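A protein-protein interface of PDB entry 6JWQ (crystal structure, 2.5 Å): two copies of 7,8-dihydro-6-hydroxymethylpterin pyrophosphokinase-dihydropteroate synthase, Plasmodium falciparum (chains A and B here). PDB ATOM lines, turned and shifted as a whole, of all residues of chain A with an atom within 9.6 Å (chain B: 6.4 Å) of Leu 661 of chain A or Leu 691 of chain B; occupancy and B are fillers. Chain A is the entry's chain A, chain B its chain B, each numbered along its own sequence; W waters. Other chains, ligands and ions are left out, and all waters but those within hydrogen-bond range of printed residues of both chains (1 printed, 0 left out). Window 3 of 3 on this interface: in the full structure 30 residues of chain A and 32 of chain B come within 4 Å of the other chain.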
ATOM      1  N   ALA A 613     -32.046 -14.313  11.441  1.00  0.00           N
ATOM      2  CA  ALA A 613     -30.609 -14.644  11.501  1.00  0.00           C
ATOM      3  C   ALA A 613     -29.741 -13.749  10.635  1.00  0.00           C
ATOM      4  O   ALA A 613     -28.607 -13.478  10.982  1.00  0.00           O
ATOM      5  CB  ALA A 613     -30.383 -16.106  11.137  1.00  0.00           C
ATOM      6  N   MET A 616     -28.110 -10.557  12.338  1.00  0.00           N
ATOM      7  CA  MET A 616     -27.117 -10.705  13.397  1.00  0.00           C
ATOM      8  C   MET A 616     -25.684 -10.827  12.912  1.00  0.00           C
ATOM      9  O   MET A 616     -25.432 -11.337  11.814  1.00  0.00           O
ATOM     10  CB  MET A 616     -27.535 -11.829  14.338  1.00  0.00           C
ATOM     11  CG  MET A 616     -28.786 -11.400  15.083  1.00  0.00           C
ATOM     12  SD  MET A 616     -29.664 -12.698  15.908  1.00  0.00           S
ATOM     13  CE  MET A 616     -31.243 -11.926  16.119  1.00  0.00           C
ATOM     14  N   LYS A 658     -24.798 -25.241  21.632  1.00  0.00           N
ATOM     15  CA  LYS A 658     -24.095 -24.762  20.434  1.00  0.00           C
ATOM     16  C   LYS A 658     -24.998 -24.578  19.207  1.00  0.00           C
ATOM     17  O   LYS A 658     -24.706 -23.746  18.343  1.00  0.00           O
ATOM     18  CB  LYS A 658     -22.883 -25.653  20.104  1.00  0.00           C
ATOM     19  CG  LYS A 658     -23.141 -27.161  20.121  1.00  0.00           C
ATOM     20  CD  LYS A 658     -21.869 -27.959  20.390  1.00  0.00           C
ATOM     21  CE  LYS A 658     -21.587 -28.105  21.883  1.00  0.00           C
ATOM     22  NZ  LYS A 658     -20.335 -28.870  22.153  1.00  0.00           N
ATOM     23  N   ASP A 659     -26.076 -25.364  19.140  1.00  0.00           N
ATOM     24  CA  ASP A 659     -27.104 -25.272  18.083  1.00  0.00           C
ATOM     25  C   ASP A 659     -28.417 -24.700  18.646  1.00  0.00           C
ATOM     26  O   ASP A 659     -29.213 -24.093  17.916  1.00  0.00           O
ATOM     27  CB  ASP A 659     -27.339 -26.655  17.443  1.00  0.00           C
ATOM     28  CG  ASP A 659     -27.975 -26.577  16.051  1.00  0.00           C
ATOM     29  OD1 ASP A 659     -27.429 -25.878  15.168  1.00  0.00           O
ATOM     30  OD2 ASP A 659     -29.012 -27.241  15.834  1.00  0.00           O
ATOM     31  N   GLN A 660     -28.620 -24.916  19.949  1.00  0.00           N
ATOM     32  CA  GLN A 660     -29.670 -24.272  20.745  1.00  0.00           C
ATOM     33  C   GLN A 660     -29.357 -22.780  20.907  1.00  0.00           C
ATOM     34  O   GLN A 660     -30.201 -22.003  21.361  1.00  0.00           O
ATOM     35  CB  GLN A 660     -29.795 -24.935  22.131  1.00  0.00           C
ATOM     36  CG  GLN A 660     -30.223 -26.406  22.139  1.00  0.00           C
ATOM     37  CD  GLN A 660     -31.690 -26.621  21.785  1.00  0.00           C
ATOM     38  OE1 GLN A 660     -32.587 -26.014  22.376  1.00  0.00           O
ATOM     39  NE2 GLN A 660     -31.940 -27.504  20.822  1.00  0.00           N
ATOM     40  N   LEU A 661     -28.130 -22.405  20.536  1.00  0.00           N
ATOM     41  CA  LEU A 661     -27.660 -21.026  20.505  1.00  0.00           C
ATOM     42  C   LEU A 661     -28.385 -20.222  19.427  1.00  0.00           C
ATOM     43  O   LEU A 661     -28.927 -19.145  19.711  1.00  0.00           O
ATOM     44  CB  LEU A 661     -26.154 -20.998  20.236  1.00  0.00           C
ATOM     45  CG  LEU A 661     -25.373 -19.874  20.908  1.00  0.00           C
ATOM     46  CD1 LEU A 661     -24.911 -20.301  22.303  1.00  0.00           C
ATOM     47  CD2 LEU A 661     -24.199 -19.460  20.030  1.00  0.00           C
ATOM     48  N   LEU A 662     -28.387 -20.759  18.202  1.00  0.00           N
ATOM     49  CA  LEU A 662     -29.014 -20.126  17.041  1.00  0.00           C
ATOM     50  C   LEU A 662     -30.527 -20.121  17.185  1.00  0.00           C
ATOM     51  O   LEU A 662     -31.187 -19.183  16.747  1.00  0.00           O
ATOM     52  CB  LEU A 662     -28.597 -20.811  15.738  1.00  0.00           C
ATOM     53  CG  LEU A 662     -27.098 -20.883  15.417  1.00  0.00           C
ATOM     54  CD1 LEU A 662     -26.513 -22.242  15.803  1.00  0.00           C
ATOM     55  CD2 LEU A 662     -26.857 -20.604  13.940  1.00  0.00           C
ATOM     56  N   TYR A 663     -31.050 -21.174  17.810  1.00  0.00           N
ATOM     57  CA  TYR A 663     -32.453 -21.291  18.225  1.00  0.00           C
ATOM     58  C   TYR A 663     -32.848 -20.157  19.206  1.00  0.00           C
ATOM     59  O   TYR A 663     -33.931 -19.583  19.081  1.00  0.00           O
ATOM     60  CB  TYR A 663     -32.662 -22.711  18.798  1.00  0.00           C
ATOM     61  CG  TYR A 663     -33.897 -23.002  19.652  1.00  0.00           C
ATOM     62  CD1 TYR A 663     -33.863 -22.838  21.055  1.00  0.00           C
ATOM     63  CD2 TYR A 663     -35.074 -23.516  19.073  1.00  0.00           C
ATOM     64  CE1 TYR A 663     -34.976 -23.134  21.845  1.00  0.00           C
ATOM     65  CE2 TYR A 663     -36.195 -23.813  19.854  1.00  0.00           C
ATOM     66  CZ  TYR A 663     -36.139 -23.622  21.236  1.00  0.00           C
ATOM     67  OH  TYR A 663     -37.239 -23.911  22.014  1.00  0.00           O
ATOM     68  N   GLN A 664     -31.954 -19.837  20.149  1.00  0.00           N
ATOM     69  CA  GLN A 664     -32.136 -18.736  21.105  1.00  0.00           C
ATOM     70  C   GLN A 664     -32.119 -17.364  20.429  1.00  0.00           C
ATOM     71  O   GLN A 664     -33.048 -16.571  20.630  1.00  0.00           O
ATOM     72  CB  GLN A 664     -31.078 -18.788  22.215  1.00  0.00           C
ATOM     73  CG  GLN A 664     -31.500 -19.503  23.491  1.00  0.00           C
ATOM     74  CD  GLN A 664     -32.055 -18.559  24.549  1.00  0.00           C
ATOM     75  OE1 GLN A 664     -31.309 -17.800  25.181  1.00  0.00           O
ATOM     76  NE2 GLN A 664     -33.369 -18.616  24.759  1.00  0.00           N
ATOM     77  N   LYS A 665     -31.072 -17.094  19.642  1.00  0.00           N
ATOM     78  CA  LYS A 665     -30.925 -15.831  18.915  1.00  0.00           C
ATOM     79  C   LYS A 665     -32.153 -15.551  18.027  1.00  0.00           C
ATOM     80  O   LYS A 665     -32.518 -14.395  17.771  1.00  0.00           O
ATOM     81  CB  LYS A 665     -29.687 -15.848  18.015  1.00  0.00           C
ATOM     82  CG  LYS A 665     -28.338 -15.929  18.698  1.00  0.00           C
ATOM     83  CD  LYS A 665     -27.274 -15.759  17.635  1.00  0.00           C
ATOM     84  CE  LYS A 665     -25.926 -15.380  18.215  1.00  0.00           C
ATOM     85  NZ  LYS A 665     -25.107 -14.654  17.200  1.00  0.00           N
ATOM     86  N   ASN A 666     -32.784 -16.625  17.575  1.00  0.00           N
ATOM     87  CA  ASN A 666     -33.877 -16.530  16.652  1.00  0.00           C
ATOM     88  C   ASN A 666     -35.129 -16.134  17.388  1.00  0.00           C
ATOM     89  O   ASN A 666     -35.854 -15.254  16.944  1.00  0.00           O
ATOM     90  CB  ASN A 666     -34.074 -17.867  15.933  1.00  0.00           C
ATOM     91  CG  ASN A 666     -34.184 -17.718  14.436  1.00  0.00           C
ATOM     92  OD1 ASN A 666     -33.475 -16.932  13.817  1.00  0.00           O
ATOM     93  ND2 ASN A 666     -35.064 -18.497  13.841  1.00  0.00           N
ATOM     94  N   ILE A 667     -35.387 -16.791  18.513  1.00  0.00           N
ATOM     95  CA  ILE A 667     -36.525 -16.451  19.358  1.00  0.00           C
ATOM     96  C   ILE A 667     -36.409 -14.993  19.825  1.00  0.00           C
ATOM     97  O   ILE A 667     -37.397 -14.268  19.780  1.00  0.00           O
ATOM     98  CB  ILE A 667     -36.658 -17.411  20.546  1.00  0.00           C
ATOM     99  CG1 ILE A 667     -36.946 -18.822  20.018  1.00  0.00           C
ATOM    100  CG2 ILE A 667     -37.752 -16.943  21.506  1.00  0.00           C
ATOM    101  CD1 ILE A 667     -36.871 -19.914  21.063  1.00  0.00           C
ATOM    102  N   CYS A 668     -35.200 -14.570  20.200  1.00  0.00           N
ATOM    103  CA  CYS A 668     -34.975 -13.240  20.741  1.00  0.00           C
ATOM    104  C   CYS A 668     -35.075 -12.154  19.665  1.00  0.00           C
ATOM    105  O   CYS A 668     -35.643 -11.075  19.916  1.00  0.00           O
ATOM    106  CB  CYS A 668     -33.659 -13.197  21.520  1.00  0.00           C
ATOM    107  SG  CYS A 668     -33.758 -14.201  23.041  1.00  0.00           S
ATOM    108  N   GLY A 669     -34.573 -12.465  18.463  1.00  0.00           N
ATOM    109  CA  GLY A 669     -34.772 -11.619  17.288  1.00  0.00           C
ATOM    110  C   GLY A 669     -36.247 -11.489  16.972  1.00  0.00           C
ATOM    111  O   GLY A 669     -36.720 -10.413  16.602  1.00  0.00           O
ATOM    112  N   ILE B 391     -24.402  -2.612  25.455  1.00  0.00           N
ATOM    113  CA  ILE B 391     -24.706  -3.641  26.433  1.00  0.00           C
ATOM    114  C   ILE B 391     -23.572  -3.710  27.440  1.00  0.00           C
ATOM    115  O   ILE B 391     -22.393  -3.854  27.063  1.00  0.00           O
ATOM    116  CB  ILE B 391     -24.869  -5.003  25.779  1.00  0.00           C
ATOM    117  CG1 ILE B 391     -26.111  -4.993  24.883  1.00  0.00           C
ATOM    118  CG2 ILE B 391     -24.920  -6.082  26.861  1.00  0.00           C
ATOM    119  CD1 ILE B 391     -26.231  -6.170  23.941  1.00  0.00           C
ATOM    120  N   GLU B 424     -20.700 -12.935  23.520  1.00  0.00           N
ATOM    121  CA  GLU B 424     -22.123 -12.732  23.371  1.00  0.00           C
ATOM    122  C   GLU B 424     -22.437 -11.287  22.950  1.00  0.00           C
ATOM    123  O   GLU B 424     -23.590 -10.972  22.668  1.00  0.00           O
ATOM    124  CB  GLU B 424     -22.856 -13.101  24.663  1.00  0.00           C
ATOM    125  CG  GLU B 424     -23.204 -14.575  24.836  1.00  0.00           C
ATOM    126  CD  GLU B 424     -23.922 -14.887  26.156  1.00  0.00           C
ATOM    127  OE1 GLU B 424     -24.606 -13.997  26.727  1.00  0.00           O
ATOM    128  OE2 GLU B 424     -23.817 -16.041  26.637  1.00  0.00           O
ATOM    129  N   GLY B 425     -21.428 -10.414  22.923  1.00  0.00           N
ATOM    130  CA  GLY B 425     -21.607  -9.038  22.447  1.00  0.00           C
ATOM    131  C   GLY B 425     -21.614  -7.855  23.436  1.00  0.00           C
ATOM    132  O   GLY B 425     -21.959  -6.739  23.023  1.00  0.00           O
ATOM    133  N   HIS B 688     -28.098  -9.074  32.616  1.00  0.00           N
ATOM    134  CA  HIS B 688     -27.642 -10.434  32.909  1.00  0.00           C
ATOM    135  C   HIS B 688     -27.576 -11.300  31.641  1.00  0.00           C
ATOM    136  O   HIS B 688     -26.786 -12.226  31.572  1.00  0.00           O
ATOM    137  CB  HIS B 688     -28.581 -11.115  33.896  1.00  0.00           C
ATOM    138  CG  HIS B 688     -28.626 -10.466  35.240  1.00  0.00           C
ATOM    139  ND1 HIS B 688     -29.662  -9.646  35.634  1.00  0.00           N
ATOM    140  CD2 HIS B 688     -27.768 -10.522  36.289  1.00  0.00           C
ATOM    141  CE1 HIS B 688     -29.441  -9.228  36.868  1.00  0.00           C
ATOM    142  NE2 HIS B 688     -28.294  -9.733  37.282  1.00  0.00           N
ATOM    143  N   ASP B 689     -28.429 -10.995  30.665  1.00  0.00           N
ATOM    144  CA  ASP B 689     -28.708 -11.870  29.529  1.00  0.00           C
ATOM    145  C   ASP B 689     -28.212 -11.214  28.243  1.00  0.00           C
ATOM    146  O   ASP B 689     -28.999 -10.666  27.480  1.00  0.00           O
ATOM    147  CB  ASP B 689     -30.205 -12.180  29.484  1.00  0.00           C
ATOM    148  CG  ASP B 689     -30.692 -12.935  30.746  1.00  0.00           C
ATOM    149  OD1 ASP B 689     -30.401 -14.135  30.862  1.00  0.00           O
ATOM    150  OD2 ASP B 689     -31.391 -12.362  31.622  1.00  0.00           O
ATOM    151  N   VAL B 690     -26.892 -11.263  28.029  1.00  0.00           N
ATOM    152  CA  VAL B 690     -26.213 -10.552  26.925  1.00  0.00           C
ATOM    153  C   VAL B 690     -26.624 -11.021  25.522  1.00  0.00           C
ATOM    154  O   VAL B 690     -27.031 -10.194  24.693  1.00  0.00           O
ATOM    155  CB  VAL B 690     -24.666 -10.564  27.078  1.00  0.00           C
ATOM    156  CG1 VAL B 690     -23.993  -9.830  25.928  1.00  0.00           C
ATOM    157  CG2 VAL B 690     -24.243  -9.920  28.388  1.00  0.00           C
ATOM    158  N   LEU B 691     -26.536 -12.334  25.268  1.00  0.00           N
ATOM    159  CA  LEU B 691     -26.933 -12.944  23.982  1.00  0.00           C
ATOM    160  C   LEU B 691     -28.346 -12.547  23.562  1.00  0.00           C
ATOM    161  O   LEU B 691     -28.570 -12.181  22.408  1.00  0.00           O
ATOM    162  CB  LEU B 691     -26.832 -14.480  24.048  1.00  0.00           C
ATOM    163  CG  LEU B 691     -27.146 -15.322  22.800  1.00  0.00           C
ATOM    164  CD1 LEU B 691     -26.049 -16.349  22.573  1.00  0.00           C
ATOM    165  CD2 LEU B 691     -28.522 -15.984  22.870  1.00  0.00           C
ATOM    166  N   GLU B 692     -29.284 -12.619  24.499  1.00  0.00           N
ATOM    167  CA  GLU B 692     -30.670 -12.284  24.221  1.00  0.00           C
ATOM    168  C   GLU B 692     -30.802 -10.799  23.893  1.00  0.00           C
ATOM    169  O   GLU B 692     -31.404 -10.445  22.876  1.00  0.00           O
ATOM    170  CB  GLU B 692     -31.567 -12.674  25.386  1.00  0.00           C
ATOM    171  CG  GLU B 692     -31.545 -14.160  25.708  1.00  0.00           C
ATOM    172  CD  GLU B 692     -30.456 -14.575  26.690  1.00  0.00           C
ATOM    173  OE1 GLU B 692     -29.268 -14.185  26.561  1.00  0.00           O
ATOM    174  OE2 GLU B 692     -30.817 -15.327  27.608  1.00  0.00           O
ATOM    175  N   THR B 693     -30.201  -9.947  24.728  1.00  0.00           N
ATOM    176  CA  THR B 693     -30.223  -8.499  24.530  1.00  0.00           C
ATOM    177  C   THR B 693     -29.593  -8.098  23.175  1.00  0.00           C
ATOM    178  O   THR B 693     -30.174  -7.297  22.428  1.00  0.00           O
ATOM    179  CB  THR B 693     -29.592  -7.780  25.752  1.00  0.00           C
ATOM    180  OG1 THR B 693     -30.348  -8.105  26.927  1.00  0.00           O
ATOM    181  CG2 THR B 693     -29.595  -6.284  25.590  1.00  0.00           C
ATOM    182  N   LYS B 694     -28.432  -8.673  22.863  1.00  0.00           N
ATOM    183  CA  LYS B 694     -27.742  -8.427  21.581  1.00  0.00           C
ATOM    184  C   LYS B 694     -28.570  -8.845  20.351  1.00  0.00           C
ATOM    185  O   LYS B 694     -28.618  -8.118  19.353  1.00  0.00           O
ATOM    186  CB  LYS B 694     -26.347  -9.083  21.555  1.00  0.00           C
ATOM    187  CG  LYS B 694     -25.449  -8.662  20.389  1.00  0.00           C
ATOM    188  CD  LYS B 694     -25.210  -7.156  20.356  1.00  0.00           C
ATOM    189  CE  LYS B 694     -23.981  -6.762  19.538  1.00  0.00           C
ATOM    190  NZ  LYS B 694     -24.186  -6.999  18.083  1.00  0.00           N
ATOM    191  N   SER B 695     -29.210 -10.006  20.440  1.00  0.00           N
ATOM    192  CA  SER B 695     -30.121 -10.481  19.401  1.00  0.00           C
ATOM    193  C   SER B 695     -31.218  -9.449  19.111  1.00  0.00           C
ATOM    194  O   SER B 695     -31.406  -9.046  17.939  1.00  0.00           O
ATOM    195  CB  SER B 695     -30.711 -11.833  19.800  1.00  0.00           C
ATOM    196  OG  SER B 695     -29.662 -12.750  20.086  1.00  0.00           O
ATOM    197  N   VAL B 696     -31.889  -8.988  20.182  1.00  0.00           N
ATOM    198  CA  VAL B 696     -32.891  -7.921  20.099  1.00  0.00           C
ATOM    199  C   VAL B 696     -32.314  -6.649  19.471  1.00  0.00           C
ATOM    200  O   VAL B 696     -32.908  -6.090  18.551  1.00  0.00           O
ATOM    201  CB  VAL B 696     -33.541  -7.630  21.464  1.00  0.00           C
ATOM    202  CG1 VAL B 696     -34.253  -6.286  21.481  1.00  0.00           C
ATOM    203  CG2 VAL B 696     -34.518  -8.737  21.821  1.00  0.00           C
HETATM  204  O   HOH W   1     -27.270 -12.627  19.023  1.00  0.00           O
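OE1 of Gln 664 of chain A lies close to OE2 of Glu 692 of chain B (3.5 Å).
The backbone carbonyl oxygen (O) of Gln 664 of chain A lies within hydrogen-bond range of the side-chain sulfur (SG) of Cys 668 of chain A (3.5 Å). OE1 of Glu 424 of chain B is in hydrogen-bond range of N of Leu 691 of chain B, 2.9 Å away. The side-chain hydroxyl (OG) of Ser 695 of chain B lies within hydrogen-bond range of the backbone carbonyl oxygen (O) of Leu 691 of chain B.
Among the printed residues, merely in contact across the chains: Met 616 of chain A with Ser 695 of chain B (3.4 Å), Leu 661 of chain A with Leu 691 of chain B (3.96 Å), Gln 664 of chain A with Leu 691 of chain B (3.9 Å), Lys 665 of chain A with Ser 695 of chain B (3.5 Å), Cys 668 of chain A with Glu 692 of chain B (3.5 Å), Cys 668 of chain A with Ser 695 of chain B (3.7 Å) and Cys 668 of chain A with Val 696 of chain B (3.2 Å).
Of the printed residues of chain B, Met 616 of chain A touches Ser 695. Of the printed residues of chain B, Leu 661 of chain A touches Leu 691. Printed residues of chain B within 4 Å of Gln 664 of chain A: Leu 691 and Glu 692. Of the printed residues of chain B, Lys 665 of chain A touches Ser 695. Of the printed residues of chain B, Cys 668 of chain A touches Glu 692, Ser 695 and Val 696. Asp 689 of chain B touches none of the printed residues of chain A. Val 690 of chain B touches none of the printed residues of chain A. Leu 691 of chain B touches just these residues of chain A: Leu 661 (3.96 Å) and Gln 664 (3.9 Å). Of the printed residues of chain A, Val 696 of chain B touches Cys 668 (3.2 Å). The nearest residue of chain A that does not touch Leu 691 of chain B is Lys 665 of chain A (4.2 Å).
Of the 14 printed residues of chain A, 5 touch a printed residue of chain B. Printed residues of chain A that touch a printed residue of chain B: Met 616, Leu 661, Gln 664, Lys 665 and Cys 668. Of the 12 printed residues of chain B, 4 touch a printed residue of chain A. Along chain B the printed residues that touch a printed residue of chain A span positions 691 to 696. Among the printed residues, 8 pairs touch across the chains.
No position is printed for both chains. Of the 8 pairs that touch across the chains among the printed residues, none has its exchanged pair printed and touching as well.
Water W1 bridges OG of Ser 695 of chain B (2.6 Å) and NZ of Lys 665 of chain A (3.5 Å).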
